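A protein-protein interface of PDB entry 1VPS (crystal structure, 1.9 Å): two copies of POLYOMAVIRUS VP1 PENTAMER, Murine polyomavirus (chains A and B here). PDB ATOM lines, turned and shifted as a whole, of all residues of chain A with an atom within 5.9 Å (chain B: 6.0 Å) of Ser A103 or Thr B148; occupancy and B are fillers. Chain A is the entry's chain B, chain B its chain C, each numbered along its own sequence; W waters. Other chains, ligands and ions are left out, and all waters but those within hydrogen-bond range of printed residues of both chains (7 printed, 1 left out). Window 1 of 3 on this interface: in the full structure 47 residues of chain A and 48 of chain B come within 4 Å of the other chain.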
ATOM      1  N   GLN A  40     -11.435  19.865   9.002  1.00  0.00           N
ATOM      2  CA  GLN A  40     -11.870  21.012   8.213  1.00  0.00           C
ATOM      3  C   GLN A  40     -11.751  20.757   6.703  1.00  0.00           C
ATOM      4  O   GLN A  40     -12.284  21.516   5.897  1.00  0.00           O
ATOM      5  CB  GLN A  40     -11.114  22.289   8.626  1.00  0.00           C
ATOM      6  CG  GLN A  40      -9.604  22.308   8.322  1.00  0.00           C
ATOM      7  CD  GLN A  40      -8.724  21.723   9.441  1.00  0.00           C
ATOM      8  OE1 GLN A  40      -9.040  20.685  10.039  1.00  0.00           O
ATOM      9  NE2 GLN A  40      -7.606  22.381   9.705  1.00  0.00           N
ATOM     10  N   TRP A  44     -13.362  17.562   0.972  1.00  0.00           N
ATOM     11  CA  TRP A  44     -12.336  18.043   0.048  1.00  0.00           C
ATOM     12  C   TRP A  44     -11.142  17.086   0.098  1.00  0.00           C
ATOM     13  O   TRP A  44     -11.112  16.140   0.897  1.00  0.00           O
ATOM     14  CB  TRP A  44     -11.814  19.420   0.505  1.00  0.00           C
ATOM     15  CG  TRP A  44     -12.859  20.442   0.843  1.00  0.00           C
ATOM     16  CD1 TRP A  44     -13.595  20.517   1.995  1.00  0.00           C
ATOM     17  CD2 TRP A  44     -13.278  21.542   0.025  1.00  0.00           C
ATOM     18  NE1 TRP A  44     -14.450  21.593   1.939  1.00  0.00           N
ATOM     19  CE2 TRP A  44     -14.275  22.240   0.744  1.00  0.00           C
ATOM     20  CE3 TRP A  44     -12.906  22.006  -1.243  1.00  0.00           C
ATOM     21  CZ2 TRP A  44     -14.908  23.380   0.232  1.00  0.00           C
ATOM     22  CZ3 TRP A  44     -13.535  23.139  -1.753  1.00  0.00           C
ATOM     23  CH2 TRP A  44     -14.526  23.812  -1.015  1.00  0.00           C
ATOM     24  N   GLY A 100     -26.086  20.083  -2.628  1.00  0.00           N
ATOM     25  CA  GLY A 100     -25.157  21.081  -2.128  1.00  0.00           C
ATOM     26  C   GLY A 100     -24.480  22.061  -3.062  1.00  0.00           C
ATOM     27  O   GLY A 100     -23.651  22.832  -2.585  1.00  0.00           O
ATOM     28  N   SER A 101     -24.840  22.100  -4.344  1.00  0.00           N
ATOM     29  CA  SER A 101     -24.177  23.027  -5.266  1.00  0.00           C
ATOM     30  C   SER A 101     -24.300  24.479  -4.810  1.00  0.00           C
ATOM     31  O   SER A 101     -23.413  25.288  -5.073  1.00  0.00           O
ATOM     32  CB  SER A 101     -24.690  22.860  -6.701  1.00  0.00           C
ATOM     33  OG  SER A 101     -26.064  23.190  -6.802  1.00  0.00           O
ATOM     34  N   GLY A 102     -25.372  24.790  -4.083  1.00  0.00           N
ATOM     35  CA  GLY A 102     -25.564  26.136  -3.573  1.00  0.00           C
ATOM     36  C   GLY A 102     -24.452  26.565  -2.619  1.00  0.00           C
ATOM     37  O   GLY A 102     -24.156  27.753  -2.500  1.00  0.00           O
ATOM     38  N   SER A 103     -23.797  25.612  -1.956  1.00  0.00           N
ATOM     39  CA  SER A 103     -22.722  25.967  -1.029  1.00  0.00           C
ATOM     40  C   SER A 103     -21.548  26.576  -1.790  1.00  0.00           C
ATOM     41  O   SER A 103     -20.721  27.286  -1.214  1.00  0.00           O
ATOM     42  CB  SER A 103     -22.255  24.746  -0.233  1.00  0.00           C
ATOM     43  OG  SER A 103     -21.594  23.805  -1.062  1.00  0.00           O
ATOM     44  N   LEU A 104     -21.488  26.319  -3.095  1.00  0.00           N
ATOM     45  CA  LEU A 104     -20.422  26.860  -3.931  1.00  0.00           C
ATOM     46  C   LEU A 104     -20.581  28.378  -4.124  1.00  0.00           C
ATOM     47  O   LEU A 104     -19.685  29.038  -4.652  1.00  0.00           O
ATOM     48  CB  LEU A 104     -20.350  26.118  -5.274  1.00  0.00           C
ATOM     49  CG  LEU A 104     -20.118  24.600  -5.184  1.00  0.00           C
ATOM     50  CD1 LEU A 104     -19.970  24.008  -6.569  1.00  0.00           C
ATOM     51  CD2 LEU A 104     -18.878  24.300  -4.359  1.00  0.00           C
ATOM     52  N   LEU A 105     -21.703  28.929  -3.662  1.00  0.00           N
ATOM     53  CA  LEU A 105     -21.954  30.368  -3.743  1.00  0.00           C
ATOM     54  C   LEU A 105     -21.210  31.127  -2.635  1.00  0.00           C
ATOM     55  O   LEU A 105     -21.300  32.353  -2.544  1.00  0.00           O
ATOM     56  CB  LEU A 105     -23.457  30.662  -3.672  1.00  0.00           C
ATOM     57  CG  LEU A 105     -24.284  30.157  -4.862  1.00  0.00           C
ATOM     58  CD1 LEU A 105     -25.768  30.273  -4.535  1.00  0.00           C
ATOM     59  CD2 LEU A 105     -23.924  30.937  -6.130  1.00  0.00           C
ATOM     60  N   ASP A 106     -20.531  30.397  -1.752  1.00  0.00           N
ATOM     61  CA  ASP A 106     -19.735  31.029  -0.701  1.00  0.00           C
ATOM     62  C   ASP A 106     -18.456  31.530  -1.369  1.00  0.00           C
ATOM     63  O   ASP A 106     -17.588  30.731  -1.747  1.00  0.00           O
ATOM     64  CB  ASP A 106     -19.399  30.015   0.407  1.00  0.00           C
ATOM     65  CG  ASP A 106     -18.307  30.509   1.384  1.00  0.00           C
ATOM     66  OD1 ASP A 106     -17.773  31.634   1.252  1.00  0.00           O
ATOM     67  OD2 ASP A 106     -17.969  29.740   2.310  1.00  0.00           O
ATOM     68  N   ARG A 258     -10.753  24.251  -5.259  1.00  0.00           N
ATOM     69  CA  ARG A 258     -10.689  25.584  -4.689  1.00  0.00           C
ATOM     70  C   ARG A 258      -9.154  25.806  -4.670  1.00  0.00           C
ATOM     71  O   ARG A 258      -8.371  24.835  -4.690  1.00  0.00           O
ATOM     72  CB  ARG A 258     -11.326  25.689  -3.304  1.00  0.00           C
ATOM     73  CG  ARG A 258     -10.614  24.991  -2.181  1.00  0.00           C
ATOM     74  CD  ARG A 258     -11.140  25.509  -0.849  1.00  0.00           C
ATOM     75  NE  ARG A 258     -10.374  24.948   0.255  1.00  0.00           N
ATOM     76  CZ  ARG A 258      -9.385  25.579   0.888  1.00  0.00           C
ATOM     77  NH1 ARG A 258      -9.035  26.821   0.551  1.00  0.00           N
ATOM     78  NH2 ARG A 258      -8.701  24.928   1.819  1.00  0.00           N
ATOM     79  N   ARG A 269     -13.055  19.321  -4.588  1.00  0.00           N
ATOM     80  CA  ARG A 269     -14.319  19.474  -3.869  1.00  0.00           C
ATOM     81  C   ARG A 269     -15.301  18.431  -4.400  1.00  0.00           C
ATOM     82  O   ARG A 269     -15.475  18.285  -5.621  1.00  0.00           O
ATOM     83  CB  ARG A 269     -14.921  20.870  -4.067  1.00  0.00           C
ATOM     84  CG  ARG A 269     -16.310  21.056  -3.429  1.00  0.00           C
ATOM     85  CD  ARG A 269     -16.342  20.564  -1.983  1.00  0.00           C
ATOM     86  NE  ARG A 269     -17.359  21.225  -1.169  1.00  0.00           N
ATOM     87  CZ  ARG A 269     -17.948  20.679  -0.105  1.00  0.00           C
ATOM     88  NH1 ARG A 269     -17.641  19.441   0.274  1.00  0.00           N
ATOM     89  NH2 ARG A 269     -18.770  21.406   0.647  1.00  0.00           N
ATOM     90  N   LEU A 271     -19.319  16.482  -3.705  1.00  0.00           N
ATOM     91  CA  LEU A 271     -20.627  16.662  -3.080  1.00  0.00           C
ATOM     92  C   LEU A 271     -21.321  15.313  -2.936  1.00  0.00           C
ATOM     93  O   LEU A 271     -21.066  14.396  -3.713  1.00  0.00           O
ATOM     94  CB  LEU A 271     -21.504  17.621  -3.900  1.00  0.00           C
ATOM     95  CG  LEU A 271     -21.129  19.108  -3.859  1.00  0.00           C
ATOM     96  CD1 LEU A 271     -22.043  19.891  -4.797  1.00  0.00           C
ATOM     97  CD2 LEU A 271     -21.225  19.648  -2.428  1.00  0.00           C
ATOM     98  N   LEU B 146     -25.758  22.217   4.185  1.00  0.00           N
ATOM     99  CA  LEU B 146     -24.457  21.770   3.673  1.00  0.00           C
ATOM    100  C   LEU B 146     -23.694  23.047   3.343  1.00  0.00           C
ATOM    101  O   LEU B 146     -24.162  23.875   2.549  1.00  0.00           O
ATOM    102  CB  LEU B 146     -24.592  20.880   2.425  1.00  0.00           C
ATOM    103  CG  LEU B 146     -23.311  20.161   1.966  1.00  0.00           C
ATOM    104  CD1 LEU B 146     -23.670  18.919   1.170  1.00  0.00           C
ATOM    105  CD2 LEU B 146     -22.414  21.075   1.141  1.00  0.00           C
ATOM    106  N   VAL B 147     -22.522  23.206   3.951  1.00  0.00           N
ATOM    107  CA  VAL B 147     -21.727  24.404   3.745  1.00  0.00           C
ATOM    108  C   VAL B 147     -20.331  24.111   3.231  1.00  0.00           C
ATOM    109  O   VAL B 147     -19.872  22.969   3.240  1.00  0.00           O
ATOM    110  CB  VAL B 147     -21.597  25.229   5.060  1.00  0.00           C
ATOM    111  CG1 VAL B 147     -22.975  25.670   5.557  1.00  0.00           C
ATOM    112  CG2 VAL B 147     -20.867  24.411   6.141  1.00  0.00           C
ATOM    113  N   THR B 148     -19.678  25.167   2.762  1.00  0.00           N
ATOM    114  CA  THR B 148     -18.313  25.094   2.266  1.00  0.00           C
ATOM    115  C   THR B 148     -17.365  24.917   3.455  1.00  0.00           C
ATOM    116  O   THR B 148     -16.447  24.099   3.403  1.00  0.00           O
ATOM    117  CB  THR B 148     -17.931  26.408   1.502  1.00  0.00           C
ATOM    118  OG1 THR B 148     -18.437  26.353   0.165  1.00  0.00           O
ATOM    119  CG2 THR B 148     -16.414  26.631   1.471  1.00  0.00           C
ATOM    120  N   ASP B 149     -17.627  25.650   4.535  1.00  0.00           N
ATOM    121  CA  ASP B 149     -16.760  25.619   5.709  1.00  0.00           C
ATOM    122  C   ASP B 149     -17.543  25.614   7.023  1.00  0.00           C
ATOM    123  O   ASP B 149     -18.195  26.606   7.370  1.00  0.00           O
ATOM    124  CB  ASP B 149     -15.841  26.855   5.664  1.00  0.00           C
ATOM    125  CG  ASP B 149     -14.643  26.764   6.617  1.00  0.00           C
ATOM    126  OD1 ASP B 149     -14.583  25.870   7.494  1.00  0.00           O
ATOM    127  OD2 ASP B 149     -13.737  27.606   6.469  1.00  0.00           O
ATOM    128  N   ALA B 150     -17.409  24.525   7.779  1.00  0.00           N
ATOM    129  CA  ALA B 150     -18.075  24.363   9.073  1.00  0.00           C
ATOM    130  C   ALA B 150     -17.563  25.369  10.109  1.00  0.00           C
ATOM    131  O   ALA B 150     -18.177  25.554  11.157  1.00  0.00           O
ATOM    132  CB  ALA B 150     -17.878  22.935   9.591  1.00  0.00           C
ATOM    133  N   THR B 152     -17.132  28.598   9.391  1.00  0.00           N
ATOM    134  CA  THR B 152     -17.666  29.925   9.075  1.00  0.00           C
ATOM    135  C   THR B 152     -18.479  30.473  10.250  1.00  0.00           C
ATOM    136  O   THR B 152     -19.320  29.773  10.826  1.00  0.00           O
ATOM    137  CB  THR B 152     -18.526  29.896   7.783  1.00  0.00           C
ATOM    138  OG1 THR B 152     -17.701  29.527   6.669  1.00  0.00           O
ATOM    139  CG2 THR B 152     -19.164  31.263   7.519  1.00  0.00           C
ATOM    140  N   TYR B 154     -21.206  32.645  11.043  1.00  0.00           N
ATOM    141  CA  TYR B 154     -22.396  33.386  10.635  1.00  0.00           C
ATOM    142  C   TYR B 154     -22.973  34.132  11.837  1.00  0.00           C
ATOM    143  O   TYR B 154     -22.839  33.673  12.976  1.00  0.00           O
ATOM    144  CB  TYR B 154     -23.469  32.429  10.102  1.00  0.00           C
ATOM    145  CG  TYR B 154     -23.078  31.679   8.850  1.00  0.00           C
ATOM    146  CD1 TYR B 154     -23.059  32.318   7.608  1.00  0.00           C
ATOM    147  CD2 TYR B 154     -22.734  30.327   8.905  1.00  0.00           C
ATOM    148  CE1 TYR B 154     -22.704  31.626   6.448  1.00  0.00           C
ATOM    149  CE2 TYR B 154     -22.376  29.622   7.754  1.00  0.00           C
ATOM    150  CZ  TYR B 154     -22.364  30.276   6.526  1.00  0.00           C
ATOM    151  OH  TYR B 154     -21.997  29.606   5.380  1.00  0.00           O
ATOM    152  N   ASP B 174     -20.952  18.678   8.400  1.00  0.00           N
ATOM    153  CA  ASP B 174     -21.803  19.692   7.768  1.00  0.00           C
ATOM    154  C   ASP B 174     -21.251  20.158   6.418  1.00  0.00           C
ATOM    155  O   ASP B 174     -21.912  20.906   5.689  1.00  0.00           O
ATOM    156  CB  ASP B 174     -22.038  20.877   8.709  1.00  0.00           C
ATOM    157  CG  ASP B 174     -22.949  20.518   9.879  1.00  0.00           C
ATOM    158  OD1 ASP B 174     -23.868  19.687   9.696  1.00  0.00           O
ATOM    159  OD2 ASP B 174     -22.751  21.058  10.988  1.00  0.00           O
ATOM    160  N   GLN B 175     -20.031  19.725   6.098  1.00  0.00           N
ATOM    161  CA  GLN B 175     -19.402  20.051   4.822  1.00  0.00           C
ATOM    162  C   GLN B 175     -19.786  19.008   3.778  1.00  0.00           C
ATOM    163  O   GLN B 175     -19.477  19.162   2.598  1.00  0.00           O
ATOM    164  CB  GLN B 175     -17.888  20.185   4.969  1.00  0.00           C
ATOM    165  CG  GLN B 175     -17.530  21.360   5.867  1.00  0.00           C
ATOM    166  CD  GLN B 175     -16.043  21.620   6.017  1.00  0.00           C
ATOM    167  OE1 GLN B 175     -15.657  22.567   6.697  1.00  0.00           O
ATOM    168  NE2 GLN B 175     -15.212  20.800   5.399  1.00  0.00           N
ATOM    169  N   VAL B 193     -28.838  30.763   0.953  1.00  0.00           N
ATOM    170  CA  VAL B 193     -28.763  29.725  -0.065  1.00  0.00           C
ATOM    171  C   VAL B 193     -27.416  28.998  -0.102  1.00  0.00           C
ATOM    172  O   VAL B 193     -27.323  27.898  -0.641  1.00  0.00           O
ATOM    173  CB  VAL B 193     -29.164  30.244  -1.477  1.00  0.00           C
ATOM    174  CG1 VAL B 193     -30.593  30.756  -1.440  1.00  0.00           C
ATOM    175  CG2 VAL B 193     -28.211  31.324  -1.960  1.00  0.00           C
ATOM    176  N   GLU B 194     -26.372  29.587   0.475  1.00  0.00           N
ATOM    177  CA  GLU B 194     -25.082  28.903   0.490  1.00  0.00           C
ATOM    178  C   GLU B 194     -25.063  27.855   1.609  1.00  0.00           C
ATOM    179  O   GLU B 194     -24.091  27.115   1.749  1.00  0.00           O
ATOM    180  CB  GLU B 194     -23.912  29.882   0.662  1.00  0.00           C
ATOM    181  CG  GLU B 194     -23.781  30.497   2.051  1.00  0.00           C
ATOM    182  CD  GLU B 194     -22.487  31.293   2.220  1.00  0.00           C
ATOM    183  OE1 GLU B 194     -22.136  32.092   1.323  1.00  0.00           O
ATOM    184  OE2 GLU B 194     -21.804  31.108   3.251  1.00  0.00           O
ATOM    185  N   ILE B 195     -26.147  27.792   2.386  1.00  0.00           N
ATOM    186  CA  ILE B 195     -26.276  26.849   3.498  1.00  0.00           C
ATOM    187  C   ILE B 195     -27.398  25.824   3.298  1.00  0.00           C
ATOM    188  O   ILE B 195     -27.191  24.619   3.479  1.00  0.00           O
ATOM    189  CB  ILE B 195     -26.605  27.584   4.837  1.00  0.00           C
ATOM    190  CG1 ILE B 195     -25.502  28.579   5.209  1.00  0.00           C
ATOM    191  CG2 ILE B 195     -26.813  26.573   5.978  1.00  0.00           C
ATOM    192  CD1 ILE B 195     -25.831  29.404   6.437  1.00  0.00           C
ATOM    193  N   HIS B 197     -30.253  23.766   1.173  1.00  0.00           N
ATOM    194  CA  HIS B 197     -30.566  23.189  -0.132  1.00  0.00           C
ATOM    195  C   HIS B 197     -31.818  22.324  -0.074  1.00  0.00           C
ATOM    196  O   HIS B 197     -32.197  21.851   0.998  1.00  0.00           O
ATOM    197  CB  HIS B 197     -29.381  22.321  -0.577  1.00  0.00           C
ATOM    198  CG  HIS B 197     -28.055  22.914  -0.230  1.00  0.00           C
ATOM    199  ND1 HIS B 197     -27.503  23.964  -0.933  1.00  0.00           N
ATOM    200  CD2 HIS B 197     -27.223  22.688   0.818  1.00  0.00           C
ATOM    201  CE1 HIS B 197     -26.398  24.368  -0.332  1.00  0.00           C
ATOM    202  NE2 HIS B 197     -26.207  23.608   0.732  1.00  0.00           N
HETATM  203  O   HOH W   1     -23.681  33.242  -0.589  1.00  0.00           O
HETATM  204  O   HOH W   2     -20.108  17.985   0.266  1.00  0.00           O
HETATM  205  O   HOH W   3     -16.932  27.984  -1.686  1.00  0.00           O
HETATM  206  O   HOH W   4     -13.614  24.565   3.412  1.00  0.00           O
HETATM  207  O   HOH W   5     -19.301  28.249   4.609  1.00  0.00           O
HETATM  208  O   HOH W   6     -18.787  23.794  -0.904  1.00  0.00           O
HETATM  209  O   HOH W   7     -28.049  23.677  -3.562  1.00  0.00           O
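NE1 of Trp A44 touches O of Thr B148 (3.5 Å). O of Gly A100 touches CE1 of His B197 (3.9 Å). Gly A102 touches Glu B194. His B197 touches Gly A102 (CE1 to C, 3.7 Å). Ser A103 touches Glu B194 (CA to O, 3.3 Å). His B197 touches Ser A103. Leu A105 touches Val B193. Glu B194 touches Leu A105 (OE1 to O, 3.96 Å). Asp A106 touches Glu B194. Leu B146 touches Arg A269 (CD2 to NH2, 3.7 Å).
Printed residues of chain A within 4 Å of Thr B148: Trp A44, Ser A103 and Asp A106. Of the printed residues of chain A, Val B147 touches Arg A269 (3.2 Å). Of the printed residues of chain A, His B197 touches Gly A100 (3.9 Å), Gly A102 (3.7 Å) and Ser A103 (3.3 Å). Leu A104 touches none of the printed residues of chain B. Leu A271 touches none of the printed residues of chain B. The nearest printed residue of chain A that does not touch Val B193 is Ser A103 (4.4 Å).
Water W2 bridges O of Gln B175 (2.7 Å) and NH1 of Arg A269 (2.9 Å). Water W7 lies within hydrogen-bond range of ND1 of His B197 (2.7 Å) and N of Gly A102 (2.9 Å). Water W1 lies within hydrogen-bond range of the side-chain carboxylate of Glu B194 and the backbone carbonyl oxygen of Leu A105. Water W6 lies within hydrogen-bond range of the side-chain hydroxyl of Thr B148 (2.8 Å), the side-chain hydroxyl of Ser A103 (2.8 Å) and the guanidinium group of Arg A269 (2.8 Å). Water W4 lies within hydrogen-bond range of O of Thr B148 (2.9 Å) and NE1 of Trp A44 (3.4 Å). Water W5 lies within hydrogen-bond range of the side-chain hydroxyl of Thr B152 (2.9 Å), the side-chain carboxylate of Asp A106 (3.0 Å), the backbone NH of Asp B149 (3.1 Å) and the side-chain hydroxyl of Tyr B154 (3.1 Å).
O of Gly A100 is in hydrogen-bond range of OG of Ser A103. N of Leu B146 sits at hydrogen-bond distance from O of Ile B195 (2.9 Å). The backbone carbonyl oxygen (O) of Asp B174 is in hydrogen-bond range of the backbone NH (N) of Val B147 (2.9 Å). N of Ala B150 lies within hydrogen-bond range of OE1 of Gln B175. The side-chain hydroxyl (OH) of Tyr B154 lies within hydrogen-bond range of the side-chain carboxylate (OE2) of Glu B194, at 2.6 Å. A ring nitrogen (NE2) of His B197 sits at hydrogen-bond distance from the backbone carbonyl oxygen of Ile B195 (3.1 Å).
Of the 13 printed residues of chain B, 7 touch a printed residue of chain A. Printed residues of chain B that touch a printed residue of chain A: Leu B146, Val B147, Thr B148, Gln B175, Val B193, Glu B194 and His B197. Among the printed residues, 18 pairs touch across the chains. Among the printed residues, no Asp or Glu carboxylate lies within 4 Å of a Lys or Arg side-chain nitrogen of the other chain.
No position is printed for both chains.
The backbone carbonyl oxygen (O) of Gln A40 lies within hydrogen-bond range of the side-chain amide nitrogen (NE2) of Gln B175 (3.1 Å). O of Ser A103 sits at hydrogen-bond distance from OG1 of Thr B148 (2.8 Å). The backbone carbonyl oxygen (O) of Val B147 lies within hydrogen-bond range of the guanidinium group (NH2) of Arg A269 (3.2 Å). NH1 of Arg A269 is in hydrogen-bond range of O of Gln B175, at 3.0 Å.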
